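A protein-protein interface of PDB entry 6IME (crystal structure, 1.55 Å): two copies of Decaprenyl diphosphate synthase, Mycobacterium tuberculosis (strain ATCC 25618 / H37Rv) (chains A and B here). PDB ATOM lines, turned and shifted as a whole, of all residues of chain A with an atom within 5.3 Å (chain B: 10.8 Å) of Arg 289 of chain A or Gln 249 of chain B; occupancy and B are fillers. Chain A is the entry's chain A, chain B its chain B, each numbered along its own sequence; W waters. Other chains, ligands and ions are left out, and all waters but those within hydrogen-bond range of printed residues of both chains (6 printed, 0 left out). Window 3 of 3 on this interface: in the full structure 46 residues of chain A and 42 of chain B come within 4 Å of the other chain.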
ATOM      1  N   ARG A  66     -16.445 -19.184   6.183  1.00  0.00           N
ATOM      2  CA  ARG A  66     -15.053 -19.507   5.981  1.00  0.00           C
ATOM      3  C   ARG A  66     -14.303 -18.343   5.371  1.00  0.00           C
ATOM      4  O   ARG A  66     -13.132 -18.504   5.023  1.00  0.00           O
ATOM      5  CB  ARG A  66     -14.906 -20.732   5.064  1.00  0.00           C
ATOM      6  CG  ARG A  66     -15.636 -21.974   5.578  1.00  0.00           C
ATOM      7  CD  ARG A  66     -15.008 -22.519   6.857  1.00  0.00           C
ATOM      8  NE  ARG A  66     -13.763 -23.243   6.608  1.00  0.00           N
ATOM      9  CZ  ARG A  66     -13.052 -23.858   7.550  1.00  0.00           C
ATOM     10  NH1 ARG A  66     -13.460 -23.840   8.810  1.00  0.00           N
ATOM     11  NH2 ARG A  66     -11.931 -24.494   7.234  1.00  0.00           N
ATOM     12  N   ALA A 262      -4.647 -13.672  14.494  1.00  0.00           N
ATOM     13  CA  ALA A 262      -4.764 -13.739  13.050  1.00  0.00           C
ATOM     14  C   ALA A 262      -4.048 -14.974  12.497  1.00  0.00           C
ATOM     15  O   ALA A 262      -3.024 -15.437  13.029  1.00  0.00           O
ATOM     16  CB  ALA A 262      -4.132 -12.478  12.434  1.00  0.00           C
ATOM     17  N   GLU A 263      -4.580 -15.467  11.386  1.00  0.00           N
ATOM     18  CA  GLU A 263      -3.859 -16.396  10.518  1.00  0.00           C
ATOM     19  C   GLU A 263      -2.860 -15.656   9.659  1.00  0.00           C
ATOM     20  O   GLU A 263      -3.225 -14.660   9.052  1.00  0.00           O
ATOM     21  CB  GLU A 263      -4.871 -17.078   9.599  1.00  0.00           C
ATOM     22  CG  GLU A 263      -5.843 -17.980  10.367  1.00  0.00           C
ATOM     23  CD  GLU A 263      -5.122 -19.124  11.032  1.00  0.00           C
ATOM     24  OE1 GLU A 263      -4.274 -19.752  10.379  1.00  0.00           O
ATOM     25  OE2 GLU A 263      -5.388 -19.375  12.227  1.00  0.00           O
ATOM     26  N   TYR A 264      -1.622 -16.153   9.553  1.00  0.00           N
ATOM     27  CA  TYR A 264      -0.630 -15.552   8.664  1.00  0.00           C
ATOM     28  C   TYR A 264      -0.548 -16.331   7.364  1.00  0.00           C
ATOM     29  O   TYR A 264      -0.427 -17.572   7.382  1.00  0.00           O
ATOM     30  CB  TYR A 264       0.749 -15.526   9.342  1.00  0.00           C
ATOM     31  CG  TYR A 264       0.846 -14.526  10.448  1.00  0.00           C
ATOM     32  CD1 TYR A 264       1.060 -13.189  10.152  1.00  0.00           C
ATOM     33  CD2 TYR A 264       0.677 -14.900  11.775  1.00  0.00           C
ATOM     34  CE1 TYR A 264       1.134 -12.225  11.146  1.00  0.00           C
ATOM     35  CE2 TYR A 264       0.741 -13.922  12.805  1.00  0.00           C
ATOM     36  CZ  TYR A 264       0.970 -12.592  12.452  1.00  0.00           C
ATOM     37  OH  TYR A 264       1.046 -11.546  13.396  1.00  0.00           O
ATOM     38  N   ILE A 265      -0.581 -15.612   6.240  1.00  0.00           N
ATOM     39  CA  ILE A 265      -0.270 -16.191   4.936  1.00  0.00           C
ATOM     40  C   ILE A 265       0.731 -15.277   4.256  1.00  0.00           C
ATOM     41  O   ILE A 265       0.386 -14.187   3.754  1.00  0.00           O
ATOM     42  CB  ILE A 265      -1.524 -16.428   4.090  1.00  0.00           C
ATOM     43  CG1 ILE A 265      -2.388 -17.476   4.781  1.00  0.00           C
ATOM     44  CG2 ILE A 265      -1.068 -16.794   2.633  1.00  0.00           C
ATOM     45  CD1 ILE A 265      -3.669 -17.892   4.013  1.00  0.00           C
ATOM     46  N   GLU A 285      -6.872 -20.398   0.765  1.00  0.00           N
ATOM     47  CA  GLU A 285      -6.049 -21.114   1.743  1.00  0.00           C
ATOM     48  C   GLU A 285      -6.568 -20.905   3.166  1.00  0.00           C
ATOM     49  O   GLU A 285      -6.678 -21.851   3.955  1.00  0.00           O
ATOM     50  CB  GLU A 285      -4.573 -20.695   1.605  1.00  0.00           C
ATOM     51  CG  GLU A 285      -3.717 -21.449   2.633  1.00  0.00           C
ATOM     52  CD  GLU A 285      -2.226 -21.215   2.518  1.00  0.00           C
ATOM     53  OE1 GLU A 285      -1.793 -20.534   1.580  1.00  0.00           O
ATOM     54  OE2 GLU A 285      -1.495 -21.740   3.411  1.00  0.00           O
ATOM     55  N   TYR A 286      -6.888 -19.665   3.518  1.00  0.00           N
ATOM     56  CA  TYR A 286      -7.490 -19.369   4.818  1.00  0.00           C
ATOM     57  C   TYR A 286      -8.729 -20.231   5.051  1.00  0.00           C
ATOM     58  O   TYR A 286      -8.913 -20.812   6.124  1.00  0.00           O
ATOM     59  CB  TYR A 286      -7.850 -17.874   4.873  1.00  0.00           C
ATOM     60  CG  TYR A 286      -8.678 -17.490   6.083  1.00  0.00           C
ATOM     61  CD1 TYR A 286     -10.053 -17.574   6.071  1.00  0.00           C
ATOM     62  CD2 TYR A 286      -8.063 -17.072   7.275  1.00  0.00           C
ATOM     63  CE1 TYR A 286     -10.806 -17.256   7.196  1.00  0.00           C
ATOM     64  CE2 TYR A 286      -8.784 -16.719   8.371  1.00  0.00           C
ATOM     65  CZ  TYR A 286     -10.175 -16.797   8.339  1.00  0.00           C
ATOM     66  OH  TYR A 286     -10.936 -16.465   9.420  1.00  0.00           O
ATOM     67  N   ALA A 287      -9.598 -20.305   4.042  1.00  0.00           N
ATOM     68  CA  ALA A 287     -10.847 -21.027   4.208  1.00  0.00           C
ATOM     69  C   ALA A 287     -10.609 -22.505   4.487  1.00  0.00           C
ATOM     70  O   ALA A 287     -11.471 -23.157   5.083  1.00  0.00           O
ATOM     71  CB  ALA A 287     -11.712 -20.843   2.963  1.00  0.00           C
ATOM     72  N   SER A 288      -9.480 -23.055   4.043  1.00  0.00           N
ATOM     73  CA  SER A 288      -9.186 -24.461   4.342  1.00  0.00           C
ATOM     74  C   SER A 288      -8.699 -24.717   5.776  1.00  0.00           C
ATOM     75  O   SER A 288      -8.674 -25.881   6.213  1.00  0.00           O
ATOM     76  CB  SER A 288      -8.141 -24.966   3.360  1.00  0.00           C
ATOM     77  OG  SER A 288      -6.863 -24.410   3.670  1.00  0.00           O
ATOM     78  N   ARG A 289      -8.318 -23.689   6.521  1.00  0.00           N
ATOM     79  CA  ARG A 289      -7.756 -23.776   7.865  1.00  0.00           C
ATOM     80  C   ARG A 289      -8.820 -23.836   8.965  1.00  0.00           C
ATOM     81  O   ARG A 289      -9.971 -23.429   8.790  1.00  0.00           O
ATOM     82  CB  ARG A 289      -6.834 -22.598   8.151  1.00  0.00           C
ATOM     83  CG  ARG A 289      -5.611 -22.609   7.303  1.00  0.00           C
ATOM     84  CD  ARG A 289      -4.798 -21.381   7.646  1.00  0.00           C
ATOM     85  NE  ARG A 289      -3.571 -21.352   6.870  1.00  0.00           N
ATOM     86  CZ  ARG A 289      -2.598 -20.459   7.076  1.00  0.00           C
ATOM     87  NH1 ARG A 289      -1.521 -20.504   6.322  1.00  0.00           N
ATOM     88  NH2 ARG A 289      -2.680 -19.556   8.043  1.00  0.00           N
ATOM     89  N   THR A 290      -8.409 -24.372  10.120  1.00  0.00           N
ATOM     90  CA  THR A 290      -9.241 -24.426  11.323  1.00  0.00           C
ATOM     91  C   THR A 290      -8.659 -23.524  12.400  1.00  0.00           C
ATOM     92  O   THR A 290      -7.488 -23.674  12.769  1.00  0.00           O
ATOM     93  CB  THR A 290      -9.323 -25.848  11.872  1.00  0.00           C
ATOM     94  OG1 THR A 290      -9.863 -26.706  10.866  1.00  0.00           O
ATOM     95  CG2 THR A 290     -10.231 -25.885  13.102  1.00  0.00           C
ATOM     96  N   ARG A 291      -9.486 -22.612  12.923  1.00  0.00           N
ATOM     97  CA  ARG A 291      -9.097 -21.686  13.975  1.00  0.00           C
ATOM     98  C   ARG A 291      -9.759 -22.120  15.270  1.00  0.00           C
ATOM     99  O   ARG A 291     -10.966 -22.378  15.287  1.00  0.00           O
ATOM    100  CB  ARG A 291      -9.540 -20.273  13.621  1.00  0.00           C
ATOM    101  CG  ARG A 291      -8.962 -19.825  12.245  1.00  0.00           C
ATOM    102  CD  ARG A 291      -9.422 -18.416  11.871  1.00  0.00           C
ATOM    103  NE  ARG A 291      -8.785 -17.403  12.698  1.00  0.00           N
ATOM    104  CZ  ARG A 291      -9.238 -16.158  12.807  1.00  0.00           C
ATOM    105  NH1 ARG A 291     -10.354 -15.795  12.175  1.00  0.00           N
ATOM    106  NH2 ARG A 291      -8.604 -15.294  13.572  1.00  0.00           N
ATOM    107  N   VAL B  74       6.042 -21.748  20.306  1.00  0.00           N
ATOM    108  CA  VAL B  74       4.685 -22.204  20.635  1.00  0.00           C
ATOM    109  C   VAL B  74       4.682 -23.722  20.439  1.00  0.00           C
ATOM    110  O   VAL B  74       4.797 -24.219  19.302  1.00  0.00           O
ATOM    111  CB  VAL B  74       3.653 -21.515  19.735  1.00  0.00           C
ATOM    112  CG1 VAL B  74       2.220 -21.979  20.049  1.00  0.00           C
ATOM    113  CG2 VAL B  74       3.752 -19.994  19.916  1.00  0.00           C
ATOM    114  N   ASP B  76       3.086 -26.634  19.955  1.00  0.00           N
ATOM    115  CA  ASP B  76       1.738 -26.949  19.495  1.00  0.00           C
ATOM    116  C   ASP B  76       1.718 -28.310  18.807  1.00  0.00           C
ATOM    117  O   ASP B  76       2.743 -28.775  18.286  1.00  0.00           O
ATOM    118  CB  ASP B  76       1.269 -25.859  18.526  1.00  0.00           C
ATOM    119  CG  ASP B  76      -0.230 -25.820  18.335  1.00  0.00           C
ATOM    120  OD1 ASP B  76      -1.009 -26.511  19.037  1.00  0.00           O
ATOM    121  OD2 ASP B  76      -0.655 -25.124  17.409  1.00  0.00           O
ATOM    122  N   GLY B  77       0.573 -28.982  18.906  1.00  0.00           N
ATOM    123  CA  GLY B  77       0.339 -30.254  18.230  1.00  0.00           C
ATOM    124  C   GLY B  77       0.393 -31.484  19.107  1.00  0.00           C
ATOM    125  O   GLY B  77       0.320 -32.600  18.577  1.00  0.00           O
ATOM    126  N   ARG B  80      -3.098 -33.586  18.915  1.00  0.00           N
ATOM    127  CA  ARG B  80      -3.262 -34.277  17.630  1.00  0.00           C
ATOM    128  C   ARG B  80      -2.280 -35.432  17.475  1.00  0.00           C
ATOM    129  O   ARG B  80      -2.619 -36.461  16.880  1.00  0.00           O
ATOM    130  CB  ARG B  80      -3.036 -33.295  16.481  1.00  0.00           C
ATOM    131  CG  ARG B  80      -4.232 -32.496  16.067  1.00  0.00           C
ATOM    132  CD  ARG B  80      -3.735 -31.388  15.138  1.00  0.00           C
ATOM    133  NE  ARG B  80      -3.124 -30.310  15.917  1.00  0.00           N
ATOM    134  CZ  ARG B  80      -2.609 -29.211  15.395  1.00  0.00           C
ATOM    135  NH1 ARG B  80      -2.561 -29.044  14.074  1.00  0.00           N
ATOM    136  NH2 ARG B  80      -2.097 -28.294  16.202  1.00  0.00           N
ATOM    137  N   PHE B 242      10.416 -16.384  16.046  1.00  0.00           N
ATOM    138  CA  PHE B 242       9.177 -16.941  16.603  1.00  0.00           C
ATOM    139  C   PHE B 242       8.895 -18.218  15.848  1.00  0.00           C
ATOM    140  O   PHE B 242       8.667 -18.189  14.638  1.00  0.00           O
ATOM    141  CB  PHE B 242       8.034 -15.926  16.418  1.00  0.00           C
ATOM    142  CG  PHE B 242       6.755 -16.283  17.127  1.00  0.00           C
ATOM    143  CD1 PHE B 242       5.998 -17.369  16.721  1.00  0.00           C
ATOM    144  CD2 PHE B 242       6.299 -15.470  18.163  1.00  0.00           C
ATOM    145  CE1 PHE B 242       4.790 -17.682  17.376  1.00  0.00           C
ATOM    146  CE2 PHE B 242       5.106 -15.761  18.821  1.00  0.00           C
ATOM    147  CZ  PHE B 242       4.335 -16.858  18.422  1.00  0.00           C
ATOM    148  N   LEU B 243       8.847 -19.333  16.561  1.00  0.00           N
ATOM    149  CA  LEU B 243       8.600 -20.655  15.990  1.00  0.00           C
ATOM    150  C   LEU B 243       7.255 -21.191  16.448  1.00  0.00           C
ATOM    151  O   LEU B 243       6.863 -21.064  17.623  1.00  0.00           O
ATOM    152  CB  LEU B 243       9.679 -21.667  16.419  1.00  0.00           C
ATOM    153  CG  LEU B 243      11.102 -21.245  16.143  1.00  0.00           C
ATOM    154  CD1 LEU B 243      12.070 -22.347  16.564  1.00  0.00           C
ATOM    155  CD2 LEU B 243      11.274 -20.915  14.644  1.00  0.00           C
ATOM    156  N   ARG B 244       6.559 -21.833  15.533  1.00  0.00           N
ATOM    157  CA  ARG B 244       5.380 -22.576  15.974  1.00  0.00           C
ATOM    158  C   ARG B 244       5.315 -23.893  15.248  1.00  0.00           C
ATOM    159  O   ARG B 244       5.468 -23.930  14.019  1.00  0.00           O
ATOM    160  CB  ARG B 244       4.105 -21.822  15.707  1.00  0.00           C
ATOM    161  CG  ARG B 244       2.931 -22.658  16.235  1.00  0.00           C
ATOM    162  CD  ARG B 244       1.764 -21.834  16.253  1.00  0.00           C
ATOM    163  NE  ARG B 244       0.583 -22.520  16.797  1.00  0.00           N
ATOM    164  CZ  ARG B 244      -0.409 -21.819  17.313  1.00  0.00           C
ATOM    165  NH1 ARG B 244      -0.297 -20.498  17.302  1.00  0.00           N
ATOM    166  NH2 ARG B 244      -1.483 -22.400  17.819  1.00  0.00           N
ATOM    167  N   THR B 245       5.100 -24.965  15.997  1.00  0.00           N
ATOM    168  CA  THR B 245       4.995 -26.299  15.444  1.00  0.00           C
ATOM    169  C   THR B 245       3.549 -26.630  15.077  1.00  0.00           C
ATOM    170  O   THR B 245       2.614 -25.879  15.370  1.00  0.00           O
ATOM    171  CB  THR B 245       5.559 -27.343  16.431  1.00  0.00           C
ATOM    172  OG1 THR B 245       4.953 -27.181  17.736  1.00  0.00           O
ATOM    173  CG2 THR B 245       7.057 -27.099  16.606  1.00  0.00           C
ATOM    174  N   SER B 246       3.388 -27.784  14.426  1.00  0.00           N
ATOM    175  CA  SER B 246       2.153 -28.481  14.078  1.00  0.00           C
ATOM    176  C   SER B 246       1.519 -27.992  12.785  1.00  0.00           C
ATOM    177  O   SER B 246       0.517 -28.582  12.364  1.00  0.00           O
ATOM    178  CB  SER B 246       1.077 -28.385  15.168  1.00  0.00           C
ATOM    179  OG  SER B 246       0.363 -27.156  15.024  1.00  0.00           O
ATOM    180  N   GLY B 247       2.122 -27.045  12.079  1.00  0.00           N
ATOM    181  CA  GLY B 247       1.550 -26.559  10.836  1.00  0.00           C
ATOM    182  C   GLY B 247       0.607 -25.378  10.979  1.00  0.00           C
ATOM    183  O   GLY B 247       0.199 -24.805   9.962  1.00  0.00           O
ATOM    184  N   GLU B 248       0.268 -24.985  12.193  1.00  0.00           N
ATOM    185  CA  GLU B 248      -0.564 -23.797  12.351  1.00  0.00           C
ATOM    186  C   GLU B 248       0.287 -22.559  12.148  1.00  0.00           C
ATOM    187  O   GLU B 248       1.424 -22.480  12.613  1.00  0.00           O
ATOM    188  CB  GLU B 248      -1.234 -23.724  13.717  1.00  0.00           C
ATOM    189  CG  GLU B 248      -2.073 -24.969  14.139  1.00  0.00           C
ATOM    190  CD  GLU B 248      -3.210 -25.286  13.187  1.00  0.00           C
ATOM    191  OE1 GLU B 248      -3.666 -24.408  12.420  1.00  0.00           O
ATOM    192  OE2 GLU B 248      -3.691 -26.450  13.207  1.00  0.00           O
ATOM    193  N   GLN B 249      -0.256 -21.592  11.426  1.00  0.00           N
ATOM    194  CA  GLN B 249       0.484 -20.384  11.076  1.00  0.00           C
ATOM    195  C   GLN B 249      -0.167 -19.180  11.736  1.00  0.00           C
ATOM    196  O   GLN B 249      -0.905 -18.417  11.108  1.00  0.00           O
ATOM    197  CB  GLN B 249       0.564 -20.266   9.537  1.00  0.00           C
ATOM    198  CG  GLN B 249       1.374 -21.472   8.966  1.00  0.00           C
ATOM    199  CD  GLN B 249       1.755 -21.310   7.531  1.00  0.00           C
ATOM    200  OE1 GLN B 249       1.361 -20.366   6.844  1.00  0.00           O
ATOM    201  NE2 GLN B 249       2.522 -22.287   7.035  1.00  0.00           N
ATOM    202  N   ARG B 250       0.040 -19.081  13.038  1.00  0.00           N
ATOM    203  CA  ARG B 250      -0.591 -18.074  13.881  1.00  0.00           C
ATOM    204  C   ARG B 250       0.299 -17.891  15.090  1.00  0.00           C
ATOM    205  O   ARG B 250       1.100 -18.779  15.421  1.00  0.00           O
ATOM    206  CB  ARG B 250      -2.038 -18.460  14.259  1.00  0.00           C
ATOM    207  CG  ARG B 250      -2.294 -19.922  14.516  1.00  0.00           C
ATOM    208  CD  ARG B 250      -3.750 -20.124  15.078  1.00  0.00           C
ATOM    209  NE  ARG B 250      -4.089 -21.516  15.303  1.00  0.00           N
ATOM    210  CZ  ARG B 250      -4.836 -22.243  14.499  1.00  0.00           C
ATOM    211  NH1 ARG B 250      -5.245 -23.449  14.887  1.00  0.00           N
ATOM    212  NH2 ARG B 250      -5.172 -21.775  13.316  1.00  0.00           N
ATOM    213  N   SER B 251       0.261 -16.697  15.675  1.00  0.00           N
ATOM    214  CA  SER B 251       1.044 -16.462  16.896  1.00  0.00           C
ATOM    215  C   SER B 251       0.242 -16.691  18.163  1.00  0.00           C
ATOM    216  O   SER B 251       0.843 -16.861  19.229  1.00  0.00           O
ATOM    217  CB  SER B 251       1.615 -15.046  16.893  1.00  0.00           C
ATOM    218  OG  SER B 251       0.539 -14.107  17.090  1.00  0.00           O
ATOM    219  N   SER B 252      -1.080 -16.701  18.060  1.00  0.00           N
ATOM    220  CA  SER B 252      -1.978 -17.009  19.198  1.00  0.00           C
ATOM    221  C   SER B 252      -1.594 -16.251  20.470  1.00  0.00           C
ATOM    222  O   SER B 252      -1.526 -16.830  21.564  1.00  0.00           O
ATOM    223  CB  SER B 252      -2.052 -18.515  19.465  1.00  0.00           C
ATOM    224  OG  SER B 252      -2.557 -19.162  18.282  1.00  0.00           O
ATOM    225  N   ASN B 253      -1.383 -14.943  20.326  1.00  0.00           N
ATOM    226  CA  ASN B 253      -1.252 -14.037  21.460  1.00  0.00           C
ATOM    227  C   ASN B 253       0.012 -14.287  22.261  1.00  0.00           C
ATOM    228  O   ASN B 253       0.134 -13.813  23.411  1.00  0.00           O
ATOM    229  CB  ASN B 253      -2.525 -14.192  22.326  1.00  0.00           C
ATOM    230  CG  ASN B 253      -2.806 -13.027  23.271  1.00  0.00           C
ATOM    231  OD1 ASN B 253      -2.432 -11.888  23.069  1.00  0.00           O
ATOM    232  ND2 ASN B 253      -3.543 -13.373  24.332  1.00  0.00           N
ATOM    233  N   TYR B 264       8.953 -14.897  11.757  1.00  0.00           N
ATOM    234  CA  TYR B 264       8.176 -16.119  11.990  1.00  0.00           C
ATOM    235  C   TYR B 264       8.695 -17.259  11.120  1.00  0.00           C
ATOM    236  O   TYR B 264       8.928 -17.071   9.917  1.00  0.00           O
ATOM    237  CB  TYR B 264       6.686 -15.906  11.666  1.00  0.00           C
ATOM    238  CG  TYR B 264       5.989 -15.066  12.702  1.00  0.00           C
ATOM    239  CD1 TYR B 264       5.968 -13.684  12.592  1.00  0.00           C
ATOM    240  CD2 TYR B 264       5.379 -15.658  13.790  1.00  0.00           C
ATOM    241  CE1 TYR B 264       5.341 -12.910  13.577  1.00  0.00           C
ATOM    242  CE2 TYR B 264       4.746 -14.893  14.779  1.00  0.00           C
ATOM    243  CZ  TYR B 264       4.731 -13.543  14.653  1.00  0.00           C
ATOM    244  OH  TYR B 264       4.093 -12.766  15.626  1.00  0.00           O
ATOM    245  N   ILE B 265       8.872 -18.435  11.731  1.00  0.00           N
ATOM    246  CA  ILE B 265       9.128 -19.675  11.011  1.00  0.00           C
ATOM    247  C   ILE B 265       8.142 -20.702  11.531  1.00  0.00           C
ATOM    248  O   ILE B 265       8.082 -20.987  12.745  1.00  0.00           O
ATOM    249  CB  ILE B 265      10.570 -20.172  11.131  1.00  0.00           C
ATOM    250  CG1 ILE B 265      11.483 -19.200  10.425  1.00  0.00           C
ATOM    251  CG2 ILE B 265      10.701 -21.575  10.437  1.00  0.00           C
ATOM    252  CD1 ILE B 265      12.966 -19.594  10.546  1.00  0.00           C
ATOM    253  N   PHE B 266       7.273 -21.161  10.636  1.00  0.00           N
ATOM    254  CA  PHE B 266       6.242 -22.125  10.963  1.00  0.00           C
ATOM    255  C   PHE B 266       6.724 -23.496  10.525  1.00  0.00           C
ATOM    256  O   PHE B 266       7.052 -23.700   9.346  1.00  0.00           O
ATOM    257  CB  PHE B 266       4.925 -21.782  10.271  1.00  0.00           C
ATOM    258  CG  PHE B 266       4.420 -20.426  10.632  1.00  0.00           C
ATOM    259  CD1 PHE B 266       4.164 -20.082  11.943  1.00  0.00           C
ATOM    260  CD2 PHE B 266       4.260 -19.459   9.621  1.00  0.00           C
ATOM    261  CE1 PHE B 266       3.708 -18.775  12.279  1.00  0.00           C
ATOM    262  CE2 PHE B 266       3.792 -18.166   9.960  1.00  0.00           C
ATOM    263  CZ  PHE B 266       3.517 -17.853  11.286  1.00  0.00           C
ATOM    264  N   GLN B 267       6.800 -24.420  11.460  1.00  0.00           N
ATOM    265  CA  GLN B 267       7.294 -25.764  11.175  1.00  0.00           C
ATOM    266  C   GLN B 267       6.143 -26.743  11.285  1.00  0.00           C
ATOM    267  O   GLN B 267       5.362 -26.695  12.241  1.00  0.00           O
ATOM    268  CB  GLN B 267       8.414 -26.129  12.147  1.00  0.00           C
ATOM    269  CG  GLN B 267       9.649 -25.191  11.969  1.00  0.00           C
ATOM    270  CD  GLN B 267      10.720 -25.381  13.024  1.00  0.00           C
ATOM    271  OE1 GLN B 267      10.561 -25.005  14.171  1.00  0.00           O
ATOM    272  NE2 GLN B 267      11.842 -25.983  12.599  1.00  0.00           N
ATOM    273  N   ASP B 268       6.063 -27.679  10.327  1.00  0.00           N
ATOM    274  CA  ASP B 268       4.883 -28.533  10.283  1.00  0.00           C
ATOM    275  C   ASP B 268       4.898 -29.666  11.315  1.00  0.00           C
ATOM    276  O   ASP B 268       3.814 -30.127  11.700  1.00  0.00           O
ATOM    277  CB  ASP B 268       4.719 -29.167   8.892  1.00  0.00           C
ATOM    278  CG  ASP B 268       4.124 -28.217   7.868  1.00  0.00           C
ATOM    279  OD1 ASP B 268       3.627 -27.126   8.238  1.00  0.00           O
ATOM    280  OD2 ASP B 268       4.113 -28.599   6.669  1.00  0.00           O
ATOM    281  N   LYS B 269       6.070 -30.083  11.791  1.00  0.00           N
ATOM    282  CA  LYS B 269       6.141 -31.189  12.749  1.00  0.00           C
ATOM    283  C   LYS B 269       5.304 -30.903  13.986  1.00  0.00           C
ATOM    284  O   LYS B 269       5.294 -29.785  14.507  1.00  0.00           O
ATOM    285  CB  LYS B 269       7.585 -31.415  13.236  1.00  0.00           C
ATOM    286  CG  LYS B 269       8.395 -32.464  12.562  1.00  0.00           C
ATOM    287  CD  LYS B 269       9.687 -32.664  13.374  1.00  0.00           C
ATOM    288  CE  LYS B 269      10.731 -33.464  12.650  1.00  0.00           C
ATOM    289  NZ  LYS B 269      11.627 -33.961  13.709  1.00  0.00           N
ATOM    290  N   GLU B 285      17.914 -21.109   9.018  1.00  0.00           N
ATOM    291  CA  GLU B 285      17.108 -20.287   8.130  1.00  0.00           C
ATOM    292  C   GLU B 285      17.124 -18.827   8.563  1.00  0.00           C
ATOM    293  O   GLU B 285      17.368 -17.928   7.752  1.00  0.00           O
ATOM    294  CB  GLU B 285      15.691 -20.854   8.037  1.00  0.00           C
ATOM    295  CG  GLU B 285      14.716 -19.934   7.324  1.00  0.00           C
ATOM    296  CD  GLU B 285      13.323 -20.535   7.187  1.00  0.00           C
ATOM    297  OE1 GLU B 285      13.151 -21.742   7.507  1.00  0.00           O
ATOM    298  OE2 GLU B 285      12.441 -19.777   6.759  1.00  0.00           O
HETATM  299  O   HOH W   1      -2.007 -15.197  15.480  1.00  0.00           O
HETATM  300  O   HOH W   2       2.553 -17.885   6.313  1.00  0.00           O
HETATM  301  O   HOH W   3      -1.932 -23.605   8.726  1.00  0.00           O
HETATM  302  O   HOH W   4      -2.998 -22.133  10.817  1.00  0.00           O
HETATM  303  O   HOH W   5       0.057 -11.918  15.769  1.00  0.00           O
HETATM  304  O   HOH W   6      -5.593 -25.198  10.408  1.00  0.00           O
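Water W5 bridges OH of Tyr 264 of chain A (2.6 Å) and OG of Ser 251 of chain B (2.6 Å). Water W1 lies within hydrogen-bond range of the backbone carbonyl oxygen (O) of Ala 262 of chain A, the backbone NH (N) of Ser 251 of chain B and the backbone NH (N) of Ser 252 of chain B. Water W3 lies within hydrogen-bond range of O of Gly 247 of chain B (2.7 Å) and NE of Arg 289 of chain A (3.3 Å). Water W6 bridges the side-chain carboxylate (OE1) of Glu 248 of chain B (2.9 Å) and the backbone NH (N) of Thr 290 of chain A (2.9 Å).
The guanidinium group of Arg 66 of chain A sits at hydrogen-bond distance from the backbone carbonyl oxygen of Arg 289 of chain A, 2.7 Å away. The guanidinium group (NH1) of Arg 289 of chain A is in salt-bridge range of the side-chain carboxylate (OE2) of Glu 285 of chain A, 3.2 Å away. NH1 of Arg 80 of chain B lies within salt-bridge range of OE2 of Glu 248 of chain B (3.0 Å). NH1 of Arg 250 of chain B lies within salt-bridge range of OE1 of Glu 248 of chain B.
Of chain B, only Gln 249 comes within 4 Å of Arg 289 of chain A. Of chain A, only Glu 263, Tyr 264 and Arg 289 come within 4 Å of Gln 249 of chain B. No residue of chain B comes within 4 Å of Ala 287 of chain A. No residue of chain B comes within 4 Å of Ser 288 of chain A. Thr 290 of chain A touches just these residues of chain B: Glu 248 (3.9 Å) and Arg 250 (3.0 Å). Of the printed residues of chain B, Ala 262 of chain A touches Arg 250. Of the printed residues of chain A, Arg 250 of chain B touches Ala 262 (3.4 Å), Glu 263 (2.6 Å), Thr 290 (3.0 Å) and Arg 291 (3.98 Å). Of the printed residues of chain A, Glu 248 of chain B touches Thr 290 (3.9 Å). Of the printed residues of chain A, Tyr 264 of chain B touches Tyr 264. Ser 252 of chain B touches none of the printed residues of chain A.
Tyr 264 of chain B touches its own counterpart, Tyr 264 of chain A. 3 positions are printed for both chains. Of the 9 pairs that touch across the chains among the printed residues, 1 has its exchanged pair printed and touching as well.
Of the 23 printed residues of chain B, 4 touch a printed residue of chain A. Hydrophobic or aromatic side chains of chain B within 4 Å of the printed part of chain A: Tyr 264. Of the 12 printed residues of chain A, 6 touch a printed residue of chain B. Among the printed residues, 9 pairs touch across the chains. Among the printed residues, Asp or Glu carboxylates within 4 Å of a Lys or Arg side-chain nitrogen of the other chain: Glu 263 of chain A with Arg 250 of chain B.
The side-chain carboxylate (OE2) of Glu 263 of chain A is in salt-bridge range of the guanidinium group (NH2) of Arg 250 of chain B (2.6 Å). N of Tyr 264 of chain A lies within hydrogen-bond range of O of Gln 249 of chain B (2.8 Å). The guanidinium group of Arg 289 of chain A lies within hydrogen-bond range of the side-chain amide oxygen of Gln 249 of chain B, 2.9 Å away. The guanidinium group (NH2) of Arg 250 of chain B sits at hydrogen-bond distance from the backbone carbonyl oxygen (O) of Thr 290 of chain A (3.0 Å).
Among the printed residues, merely in contact across the chains: Ala 262 of chain A with Arg 250 of chain B (3.4 Å), Glu 263 of chain A with Gln 249 of chain B (3.6 Å), Tyr 264 of chain A with Tyr 264 of chain B (3.97 Å), Thr 290 of chain A with Glu 248 of chain B (3.9 Å) and Arg 291 of chain A with Arg 250 of chain B (3.98 Å).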
